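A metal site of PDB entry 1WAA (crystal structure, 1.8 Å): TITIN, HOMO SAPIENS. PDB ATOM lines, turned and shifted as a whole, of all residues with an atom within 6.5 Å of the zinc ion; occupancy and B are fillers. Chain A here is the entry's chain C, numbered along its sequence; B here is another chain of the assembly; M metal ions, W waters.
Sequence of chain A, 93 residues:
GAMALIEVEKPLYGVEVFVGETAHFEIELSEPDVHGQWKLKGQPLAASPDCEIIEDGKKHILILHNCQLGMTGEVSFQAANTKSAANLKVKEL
NZ of Lys 59 of chain B is in salt-bridge range of OE1 of Glu 52 (3.1 Å).
The backbone carbonyl oxygen (O) of Glu 52 lies within hydrogen-bond range of the backbone NH (N) of Ile 63.
The side-chain carboxylate (OE1) of Glu 26 of chain B sits close to the side-chain amino group (NZ) of Lys 59 of chain B (2.9 Å).
The zinc ion is bound by OE2 of Glu 52, OE1 of Glu 26 of chain B, NE2 of His 65, water W1 and OE2 of Glu 26 of chain B.
NZ of Lys 59 of chain B touches the zinc ion (3.98 Å).
Four residues have an atom within 4 Å of the zinc ion: Glu 52, His 65, Glu 26 of chain B and Lys 59 of chain B.
The nearest printed residue that does not touch the zinc ion is Ile 63 (4.1 Å).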
ATOM      1  N   THR A  22      14.960  23.140  -8.778  1.00  0.00           N
ATOM      2  CA  THR A  22      14.897  21.862  -8.068  1.00  0.00           C
ATOM      3  C   THR A  22      13.642  21.763  -7.183  1.00  0.00           C
ATOM      4  O   THR A  22      13.141  22.749  -6.617  1.00  0.00           O
ATOM      5  CB  THR A  22      16.231  21.512  -7.298  1.00  0.00           C
ATOM      6  OG1 THR A  22      16.013  21.253  -5.905  1.00  0.00           O
ATOM      7  CG2 THR A  22      17.284  22.578  -7.416  1.00  0.00           C
ATOM      8  N   PRO A  49      23.116  12.240  -9.823  1.00  0.00           N
ATOM      9  CA  PRO A  49      23.391  13.604  -9.415  1.00  0.00           C
ATOM     10  C   PRO A  49      22.151  14.502  -9.347  1.00  0.00           C
ATOM     11  O   PRO A  49      22.076  15.377  -8.444  1.00  0.00           O
ATOM     12  CB  PRO A  49      24.434  14.080 -10.403  1.00  0.00           C
ATOM     13  CG  PRO A  49      24.944  12.862 -11.120  1.00  0.00           C
ATOM     14  CD  PRO A  49      23.930  11.780 -10.958  1.00  0.00           C
ATOM     15  N   GLU A  52      18.443  12.742  -5.763  1.00  0.00           N
ATOM     16  CA  GLU A  52      19.036  12.416  -4.476  1.00  0.00           C
ATOM     17  C   GLU A  52      17.966  11.952  -3.491  1.00  0.00           C
ATOM     18  O   GLU A  52      16.926  12.590  -3.320  1.00  0.00           O
ATOM     19  CB  GLU A  52      19.803  13.651  -3.976  1.00  0.00           C
ATOM     20  CG  GLU A  52      20.801  14.182  -5.027  1.00  0.00           C
ATOM     21  CD  GLU A  52      21.509  15.454  -4.601  1.00  0.00           C
ATOM     22  OE1 GLU A  52      22.776  15.514  -4.672  1.00  0.00           O
ATOM     23  OE2 GLU A  52      20.840  16.420  -4.159  1.00  0.00           O
ATOM     24  N   ILE A  63      15.181  14.861  -3.551  1.00  0.00           N
ATOM     25  CA  ILE A  63      15.580  16.100  -4.212  1.00  0.00           C
ATOM     26  C   ILE A  63      15.734  15.805  -5.691  1.00  0.00           C
ATOM     27  O   ILE A  63      16.515  14.918  -6.087  1.00  0.00           O
ATOM     28  CB  ILE A  63      16.904  16.631  -3.646  1.00  0.00           C
ATOM     29  CG1 ILE A  63      16.786  16.868  -2.123  1.00  0.00           C
ATOM     30  CG2 ILE A  63      17.334  17.919  -4.381  1.00  0.00           C
ATOM     31  CD1 ILE A  63      18.042  17.386  -1.433  1.00  0.00           C
ATOM     32  N   HIS A  65      16.861  17.658  -9.075  1.00  0.00           N
ATOM     33  CA  HIS A  65      17.472  18.849  -9.662  1.00  0.00           C
ATOM     34  C   HIS A  65      17.121  18.959 -11.114  1.00  0.00           C
ATOM     35  O   HIS A  65      16.776  17.967 -11.726  1.00  0.00           O
ATOM     36  CB  HIS A  65      18.990  18.762  -9.560  1.00  0.00           C
ATOM     37  CG  HIS A  65      19.480  18.935  -8.154  1.00  0.00           C
ATOM     38  ND1 HIS A  65      19.275  20.095  -7.449  1.00  0.00           N
ATOM     39  CD2 HIS A  65      20.152  18.098  -7.333  1.00  0.00           C
ATOM     40  CE1 HIS A  65      19.818  19.959  -6.248  1.00  0.00           C
ATOM     41  NE2 HIS A  65      20.348  18.759  -6.160  1.00  0.00           N
ATOM     42  N   LYS B  10      29.437  21.234  -2.605  1.00  0.00           N
ATOM     43  CA  LYS B  10      28.349  21.902  -3.340  1.00  0.00           C
ATOM     44  C   LYS B  10      27.768  22.945  -2.434  1.00  0.00           C
ATOM     45  O   LYS B  10      27.224  22.612  -1.370  1.00  0.00           O
ATOM     46  CB  LYS B  10      27.252  20.920  -3.779  1.00  0.00           C
ATOM     47  CG  LYS B  10      27.783  19.747  -4.591  1.00  0.00           C
ATOM     48  CD  LYS B  10      26.701  19.029  -5.374  1.00  0.00           C
ATOM     49  CE  LYS B  10      27.306  17.895  -6.205  1.00  0.00           C
ATOM     50  NZ  LYS B  10      28.073  16.954  -5.333  1.00  0.00           N
ATOM     51  N   GLU B  26      20.321  23.278   0.782  1.00  0.00           N
ATOM     52  CA  GLU B  26      21.096  22.034   0.668  1.00  0.00           C
ATOM     53  C   GLU B  26      22.548  22.399   0.431  1.00  0.00           C
ATOM     54  O   GLU B  26      22.893  23.172  -0.499  1.00  0.00           O
ATOM     55  CB  GLU B  26      20.526  21.165  -0.461  1.00  0.00           C
ATOM     56  CG  GLU B  26      21.263  19.826  -0.723  1.00  0.00           C
ATOM     57  CD  GLU B  26      21.228  19.412  -2.166  1.00  0.00           C
ATOM     58  OE1 GLU B  26      21.826  18.373  -2.467  1.00  0.00           O
ATOM     59  OE2 GLU B  26      20.661  20.139  -3.004  1.00  0.00           O
ATOM     60  N   LYS B  59      25.608  15.356   3.282  1.00  0.00           N
ATOM     61  CA  LYS B  59      24.616  16.394   2.965  1.00  0.00           C
ATOM     62  C   LYS B  59      23.925  16.984   4.182  1.00  0.00           C
ATOM     63  O   LYS B  59      23.542  16.267   5.106  1.00  0.00           O
ATOM     64  CB  LYS B  59      23.519  15.854   2.071  1.00  0.00           C
ATOM     65  CG  LYS B  59      23.960  15.271   0.802  1.00  0.00           C
ATOM     66  CD  LYS B  59      22.763  14.818  -0.011  1.00  0.00           C
ATOM     67  CE  LYS B  59      22.429  15.846  -1.032  1.00  0.00           C
ATOM     68  NZ  LYS B  59      23.662  16.182  -1.808  1.00  0.00           N
HETATM   69 ZN    ZN M   1      21.468  18.180  -4.466  1.00  0.00          ZN
HETATM   70  O   HOH W   1      23.467  18.524  -5.170  1.00  0.00           O
